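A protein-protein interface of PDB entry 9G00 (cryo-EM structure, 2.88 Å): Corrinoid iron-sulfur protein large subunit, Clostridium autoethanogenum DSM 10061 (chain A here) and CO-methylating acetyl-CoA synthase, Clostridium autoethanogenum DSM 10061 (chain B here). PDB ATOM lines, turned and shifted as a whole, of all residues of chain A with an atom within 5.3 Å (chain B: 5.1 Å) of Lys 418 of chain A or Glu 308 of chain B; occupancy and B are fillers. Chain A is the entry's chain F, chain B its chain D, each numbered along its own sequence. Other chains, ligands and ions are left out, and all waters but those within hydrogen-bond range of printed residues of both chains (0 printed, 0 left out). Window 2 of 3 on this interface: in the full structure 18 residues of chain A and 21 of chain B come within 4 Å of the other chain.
The backbone carbonyl oxygen (O) of Glu 306 of chain B lies close to the backbone carbonyl oxygen (O) of Ala 415 of chain A, at 3.5 Å. The backbone NH of Gly 419 of chain A is in hydrogen-bond range of the backbone carbonyl oxygen of Gly 307 of chain B (2.8 Å).
OE2 of Glu 308 of chain B sits at hydrogen-bond distance from N of Gly 394 of chain B (2.7 Å).
Gly 307 of chain B touches Ala 415 of chain A. Gly 307 of chain B touches Val 416 of chain A. Arg 309 of chain B touches Val 416 of chain A. Lys 418 of chain A touches Gly 307 of chain B. Lys 418 of chain A touches Glu 308 of chain B. Arg 309 of chain B touches Gly 419 of chain A. Glu 420 of chain A touches Arg 309 of chain B (N to NH2, 3.9 Å).
Printed residues of chain B that touch a printed residue of chain A: Glu 306, Gly 307, Glu 308 and Arg 309.
Of the printed residues of chain B, Val 416 of chain A touches Gly 307 (3.7 Å) and Arg 309 (3.5 Å). Of the printed residues of chain B, Lys 418 of chain A touches Gly 307 and Glu 308. Printed residues of chain B within 4 Å of Gly 419 of chain A: Gly 307 and Arg 309. Printed residues of chain B within 4 Å of Glu 420 of chain A: Arg 309 (3.9 Å). Ile 430 of chain A touches none of the printed residues of chain B. Printed residues of chain A within 4 Å of Glu 306 of chain B: Ala 415 (3.1 Å). Glu 308 of chain B touches just one residue of chain A: Lys 418 (3.5 Å). Printed residues of chain A within 4 Å of Arg 309 of chain B: Val 416, Gly 419 and Glu 420. The nearest printed residue of chain B that does not touch Lys 418 of chain A is Arg 309 of chain B (4.9 Å). The nearest residue of chain A that does not touch Glu 308 of chain B is Gly 419 of chain A (4.5 Å).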
ATOM      1  N   ILE A 410     -20.847   0.222  -3.006  1.00  0.00           N
ATOM      2  CA  ILE A 410     -20.140   1.446  -3.372  1.00  0.00           C
ATOM      3  C   ILE A 410     -20.813   2.021  -4.611  1.00  0.00           C
ATOM      4  O   ILE A 410     -21.599   1.333  -5.286  1.00  0.00           O
ATOM      5  CB  ILE A 410     -18.635   1.189  -3.607  1.00  0.00           C
ATOM      6  CG1 ILE A 410     -18.443   0.260  -4.810  1.00  0.00           C
ATOM      7  CG2 ILE A 410     -18.019   0.587  -2.357  1.00  0.00           C
ATOM      8  CD1 ILE A 410     -17.004  -0.051  -5.137  1.00  0.00           C
ATOM      9  N   VAL A 414     -17.553   4.172  -9.739  1.00  0.00           N
ATOM     10  CA  VAL A 414     -16.251   3.890  -9.150  1.00  0.00           C
ATOM     11  C   VAL A 414     -15.933   2.429  -9.440  1.00  0.00           C
ATOM     12  O   VAL A 414     -16.554   1.524  -8.877  1.00  0.00           O
ATOM     13  CB  VAL A 414     -16.245   4.188  -7.650  1.00  0.00           C
ATOM     14  CG1 VAL A 414     -15.061   3.533  -6.965  1.00  0.00           C
ATOM     15  CG2 VAL A 414     -16.208   5.682  -7.441  1.00  0.00           C
ATOM     16  N   ALA A 415     -14.977   2.195 -10.336  1.00  0.00           N
ATOM     17  CA  ALA A 415     -14.726   0.867 -10.876  1.00  0.00           C
ATOM     18  C   ALA A 415     -13.441   0.246 -10.346  1.00  0.00           C
ATOM     19  O   ALA A 415     -13.471  -0.845  -9.771  1.00  0.00           O
ATOM     20  CB  ALA A 415     -14.689   0.948 -12.405  1.00  0.00           C
ATOM     21  N   VAL A 416     -12.304   0.917 -10.529  1.00  0.00           N
ATOM     22  CA  VAL A 416     -11.021   0.336 -10.158  1.00  0.00           C
ATOM     23  C   VAL A 416     -10.873   0.195  -8.648  1.00  0.00           C
ATOM     24  O   VAL A 416     -10.091  -0.643  -8.184  1.00  0.00           O
ATOM     25  CB  VAL A 416      -9.863   1.170 -10.738  1.00  0.00           C
ATOM     26  CG1 VAL A 416      -8.548   0.410 -10.622  1.00  0.00           C
ATOM     27  CG2 VAL A 416     -10.130   1.528 -12.193  1.00  0.00           C
ATOM     28  N   LEU A 417     -11.602   0.988  -7.859  1.00  0.00           N
ATOM     29  CA  LEU A 417     -11.470   0.906  -6.408  1.00  0.00           C
ATOM     30  C   LEU A 417     -12.013  -0.400  -5.846  1.00  0.00           C
ATOM     31  O   LEU A 417     -11.687  -0.745  -4.706  1.00  0.00           O
ATOM     32  CB  LEU A 417     -12.178   2.082  -5.734  1.00  0.00           C
ATOM     33  CG  LEU A 417     -11.629   3.492  -5.966  1.00  0.00           C
ATOM     34  CD1 LEU A 417     -12.331   4.485  -5.054  1.00  0.00           C
ATOM     35  CD2 LEU A 417     -10.126   3.556  -5.744  1.00  0.00           C
ATOM     36  N   LYS A 418     -12.825  -1.135  -6.609  1.00  0.00           N
ATOM     37  CA  LYS A 418     -13.413  -2.363  -6.082  1.00  0.00           C
ATOM     38  C   LYS A 418     -12.331  -3.362  -5.692  1.00  0.00           C
ATOM     39  O   LYS A 418     -12.416  -4.001  -4.637  1.00  0.00           O
ATOM     40  CB  LYS A 418     -14.370  -2.971  -7.106  1.00  0.00           C
ATOM     41  CG  LYS A 418     -14.875  -4.360  -6.742  1.00  0.00           C
ATOM     42  CD  LYS A 418     -14.147  -5.433  -7.537  1.00  0.00           C
ATOM     43  CE  LYS A 418     -14.685  -6.823  -7.236  1.00  0.00           C
ATOM     44  NZ  LYS A 418     -14.045  -7.858  -8.093  1.00  0.00           N
ATOM     45  N   GLY A 419     -11.324  -3.537  -6.546  1.00  0.00           N
ATOM     46  CA  GLY A 419     -10.187  -4.358  -6.164  1.00  0.00           C
ATOM     47  C   GLY A 419      -9.354  -3.720  -5.068  1.00  0.00           C
ATOM     48  O   GLY A 419      -8.878  -4.405  -4.159  1.00  0.00           O
ATOM     49  N   GLU A 420      -9.158  -2.401  -5.144  1.00  0.00           N
ATOM     50  CA  GLU A 420      -8.380  -1.704  -4.123  1.00  0.00           C
ATOM     51  C   GLU A 420      -9.094  -1.713  -2.777  1.00  0.00           C
ATOM     52  O   GLU A 420      -8.453  -1.872  -1.732  1.00  0.00           O
ATOM     53  CB  GLU A 420      -8.096  -0.272  -4.569  1.00  0.00           C
ATOM     54  CG  GLU A 420      -7.261   0.531  -3.584  1.00  0.00           C
ATOM     55  CD  GLU A 420      -6.974   1.933  -4.080  1.00  0.00           C
ATOM     56  OE1 GLU A 420      -7.258   2.211  -5.264  1.00  0.00           O
ATOM     57  OE2 GLU A 420      -6.469   2.758  -3.289  1.00  0.00           O
ATOM     58  N   LEU A 421     -10.417  -1.533  -2.777  1.00  0.00           N
ATOM     59  CA  LEU A 421     -11.166  -1.585  -1.524  1.00  0.00           C
ATOM     60  C   LEU A 421     -11.059  -2.959  -0.883  1.00  0.00           C
ATOM     61  O   LEU A 421     -10.886  -3.073   0.336  1.00  0.00           O
ATOM     62  CB  LEU A 421     -12.634  -1.229  -1.761  1.00  0.00           C
ATOM     63  CG  LEU A 421     -13.088   0.139  -1.254  1.00  0.00           C
ATOM     64  CD1 LEU A 421     -12.400   1.236  -2.023  1.00  0.00           C
ATOM     65  CD2 LEU A 421     -14.591   0.271  -1.371  1.00  0.00           C
ATOM     66  N   GLU A 422     -11.154  -4.017  -1.688  1.00  0.00           N
ATOM     67  CA  GLU A 422     -11.068  -5.367  -1.146  1.00  0.00           C
ATOM     68  C   GLU A 422      -9.731  -5.604  -0.454  1.00  0.00           C
ATOM     69  O   GLU A 422      -9.664  -6.361   0.521  1.00  0.00           O
ATOM     70  CB  GLU A 422     -11.281  -6.391  -2.258  1.00  0.00           C
ATOM     71  CG  GLU A 422     -11.193  -7.836  -1.793  1.00  0.00           C
ATOM     72  CD  GLU A 422     -12.202  -8.162  -0.710  1.00  0.00           C
ATOM     73  OE1 GLU A 422     -13.318  -7.602  -0.747  1.00  0.00           O
ATOM     74  OE2 GLU A 422     -11.877  -8.973   0.181  1.00  0.00           O
ATOM     75  N   ILE A 430     -17.479  -6.391  -0.983  1.00  0.00           N
ATOM     76  CA  ILE A 430     -17.722  -5.209  -1.800  1.00  0.00           C
ATOM     77  C   ILE A 430     -18.652  -5.587  -2.941  1.00  0.00           C
ATOM     78  O   ILE A 430     -18.469  -6.626  -3.588  1.00  0.00           O
ATOM     79  CB  ILE A 430     -16.404  -4.626  -2.341  1.00  0.00           C
ATOM     80  CG1 ILE A 430     -15.431  -4.326  -1.200  1.00  0.00           C
ATOM     81  CG2 ILE A 430     -16.672  -3.367  -3.148  1.00  0.00           C
ATOM     82  CD1 ILE A 430     -15.921  -3.290  -0.216  1.00  0.00           C
ATOM     83  N   ILE A 432     -20.203  -3.824  -6.445  1.00  0.00           N
ATOM     84  CA  ILE A 432     -20.020  -2.717  -7.375  1.00  0.00           C
ATOM     85  C   ILE A 432     -21.223  -2.676  -8.307  1.00  0.00           C
ATOM     86  O   ILE A 432     -21.557  -3.678  -8.952  1.00  0.00           O
ATOM     87  CB  ILE A 432     -18.701  -2.845  -8.155  1.00  0.00           C
ATOM     88  CG1 ILE A 432     -18.533  -1.649  -9.087  1.00  0.00           C
ATOM     89  CG2 ILE A 432     -18.659  -4.149  -8.931  1.00  0.00           C
ATOM     90  CD1 ILE A 432     -17.155  -1.520  -9.662  1.00  0.00           C
ATOM     91  N   PHE B 305     -17.161  -5.807 -13.792  1.00  0.00           N
ATOM     92  CA  PHE B 305     -16.042  -6.706 -13.539  1.00  0.00           C
ATOM     93  C   PHE B 305     -14.687  -6.015 -13.625  1.00  0.00           C
ATOM     94  O   PHE B 305     -13.709  -6.540 -13.082  1.00  0.00           O
ATOM     95  CB  PHE B 305     -16.089  -7.882 -14.512  1.00  0.00           C
ATOM     96  CG  PHE B 305     -17.245  -8.820 -14.283  1.00  0.00           C
ATOM     97  CD1 PHE B 305     -17.990  -8.775 -13.111  1.00  0.00           C
ATOM     98  CD2 PHE B 305     -17.583  -9.758 -15.242  1.00  0.00           C
ATOM     99  CE1 PHE B 305     -19.047  -9.642 -12.907  1.00  0.00           C
ATOM    100  CE2 PHE B 305     -18.637 -10.627 -15.044  1.00  0.00           C
ATOM    101  CZ  PHE B 305     -19.371 -10.569 -13.876  1.00  0.00           C
ATOM    102  N   GLU B 306     -14.601  -4.854 -14.267  1.00  0.00           N
ATOM    103  CA  GLU B 306     -13.335  -4.137 -14.312  1.00  0.00           C
ATOM    104  C   GLU B 306     -12.951  -3.677 -12.912  1.00  0.00           C
ATOM    105  O   GLU B 306     -13.803  -3.483 -12.041  1.00  0.00           O
ATOM    106  CB  GLU B 306     -13.420  -2.930 -15.246  1.00  0.00           C
ATOM    107  CG  GLU B 306     -14.343  -1.834 -14.759  1.00  0.00           C
ATOM    108  CD  GLU B 306     -14.122  -0.523 -15.475  1.00  0.00           C
ATOM    109  OE1 GLU B 306     -13.039  -0.345 -16.067  1.00  0.00           O
ATOM    110  OE2 GLU B 306     -15.032   0.332 -15.445  1.00  0.00           O
ATOM    111  N   GLY B 307     -11.651  -3.511 -12.697  1.00  0.00           N
ATOM    112  CA  GLY B 307     -11.154  -3.157 -11.388  1.00  0.00           C
ATOM    113  C   GLY B 307     -11.008  -4.315 -10.431  1.00  0.00           C
ATOM    114  O   GLY B 307     -10.678  -4.090  -9.260  1.00  0.00           O
ATOM    115  N   GLU B 308     -11.256  -5.543 -10.878  1.00  0.00           N
ATOM    116  CA  GLU B 308     -11.067  -6.709 -10.034  1.00  0.00           C
ATOM    117  C   GLU B 308      -9.575  -6.954  -9.813  1.00  0.00           C
ATOM    118  O   GLU B 308      -8.712  -6.274 -10.374  1.00  0.00           O
ATOM    119  CB  GLU B 308     -11.721  -7.935 -10.665  1.00  0.00           C
ATOM    120  CG  GLU B 308     -11.166  -8.290 -12.037  1.00  0.00           C
ATOM    121  CD  GLU B 308     -11.476  -9.716 -12.437  1.00  0.00           C
ATOM    122  OE1 GLU B 308     -11.256 -10.625 -11.610  1.00  0.00           O
ATOM    123  OE2 GLU B 308     -11.942  -9.928 -13.576  1.00  0.00           O
ATOM    124  N   ARG B 309      -9.270  -7.951  -8.983  1.00  0.00           N
ATOM    125  CA  ARG B 309      -7.898  -8.383  -8.751  1.00  0.00           C
ATOM    126  C   ARG B 309      -7.820  -9.893  -8.892  1.00  0.00           C
ATOM    127  O   ARG B 309      -8.577 -10.621  -8.242  1.00  0.00           O
ATOM    128  CB  ARG B 309      -7.391  -7.954  -7.369  1.00  0.00           C
ATOM    129  CG  ARG B 309      -7.322  -6.448  -7.171  1.00  0.00           C
ATOM    130  CD  ARG B 309      -6.395  -5.762  -8.168  1.00  0.00           C
ATOM    131  NE  ARG B 309      -6.871  -4.425  -8.503  1.00  0.00           N
ATOM    132  CZ  ARG B 309      -6.388  -3.296  -8.002  1.00  0.00           C
ATOM    133  NH1 ARG B 309      -5.379  -3.292  -7.147  1.00  0.00           N
ATOM    134  NH2 ARG B 309      -6.930  -2.140  -8.373  1.00  0.00           N
ATOM    135  N   ILE B 310      -6.906 -10.356  -9.736  1.00  0.00           N
ATOM    136  CA  ILE B 310      -6.621 -11.777  -9.876  1.00  0.00           C
ATOM    137  C   ILE B 310      -5.539 -12.141  -8.870  1.00  0.00           C
ATOM    138  O   ILE B 310      -4.495 -11.480  -8.800  1.00  0.00           O
ATOM    139  CB  ILE B 310      -6.187 -12.119 -11.312  1.00  0.00           C
ATOM    140  CG1 ILE B 310      -7.334 -11.838 -12.286  1.00  0.00           C
ATOM    141  CG2 ILE B 310      -5.760 -13.583 -11.412  1.00  0.00           C
ATOM    142  CD1 ILE B 310      -6.971 -12.026 -13.742  1.00  0.00           C
ATOM    143  N   ILE B 392     -14.290  -8.007 -18.919  1.00  0.00           N
ATOM    144  CA  ILE B 392     -14.403  -9.460 -18.892  1.00  0.00           C
ATOM    145  C   ILE B 392     -13.875  -9.964 -17.558  1.00  0.00           C
ATOM    146  O   ILE B 392     -12.813  -9.530 -17.095  1.00  0.00           O
ATOM    147  CB  ILE B 392     -13.631 -10.098 -20.059  1.00  0.00           C
ATOM    148  CG1 ILE B 392     -13.851  -9.317 -21.357  1.00  0.00           C
ATOM    149  CG2 ILE B 392     -14.066 -11.546 -20.236  1.00  0.00           C
ATOM    150  CD1 ILE B 392     -12.922  -9.729 -22.478  1.00  0.00           C
ATOM    151  N   GLU B 393     -14.615 -10.877 -16.933  1.00  0.00           N
ATOM    152  CA  GLU B 393     -14.146 -11.493 -15.699  1.00  0.00           C
ATOM    153  C   GLU B 393     -12.880 -12.297 -15.957  1.00  0.00           C
ATOM    154  O   GLU B 393     -12.776 -13.024 -16.948  1.00  0.00           O
ATOM    155  CB  GLU B 393     -15.225 -12.399 -15.109  1.00  0.00           C
ATOM    156  CG  GLU B 393     -14.674 -13.596 -14.340  1.00  0.00           C
ATOM    157  CD  GLU B 393     -15.686 -14.192 -13.393  1.00  0.00           C
ATOM    158  OE1 GLU B 393     -16.374 -13.418 -12.695  1.00  0.00           O
ATOM    159  OE2 GLU B 393     -15.797 -15.436 -13.345  1.00  0.00           O
ATOM    160  N   GLY B 394     -11.915 -12.167 -15.051  1.00  0.00           N
ATOM    161  CA  GLY B 394     -10.672 -12.895 -15.151  1.00  0.00           C
ATOM    162  C   GLY B 394      -9.689 -12.337 -16.154  1.00  0.00           C
ATOM    163  O   GLY B 394      -8.615 -12.925 -16.336  1.00  0.00           O
ATOM    164  N   VAL B 395     -10.018 -11.228 -16.811  1.00  0.00           N
ATOM    165  CA  VAL B 395      -9.139 -10.588 -17.780  1.00  0.00           C
ATOM    166  C   VAL B 395      -8.998  -9.129 -17.377  1.00  0.00           C
ATOM    167  O   VAL B 395     -10.002  -8.419 -17.244  1.00  0.00           O
ATOM    168  CB  VAL B 395      -9.678 -10.702 -19.215  1.00  0.00           C
ATOM    169  CG1 VAL B 395      -8.759  -9.976 -20.185  1.00  0.00           C
ATOM    170  CG2 VAL B 395      -9.837 -12.162 -19.610  1.00  0.00           C
ATOM    171  N   MET B 396      -7.762  -8.685 -17.179  1.00  0.00           N
ATOM    172  CA  MET B 396      -7.479  -7.308 -16.808  1.00  0.00           C
ATOM    173  C   MET B 396      -6.397  -6.765 -17.725  1.00  0.00           C
ATOM    174  O   MET B 396      -5.319  -7.356 -17.837  1.00  0.00           O
ATOM    175  CB  MET B 396      -7.049  -7.208 -15.348  1.00  0.00           C
ATOM    176  CG  MET B 396      -6.146  -8.336 -14.906  1.00  0.00           C
ATOM    177  SD  MET B 396      -5.617  -8.185 -13.194  1.00  0.00           S
ATOM    178  CE  MET B 396      -7.200  -8.064 -12.372  1.00  0.00           C
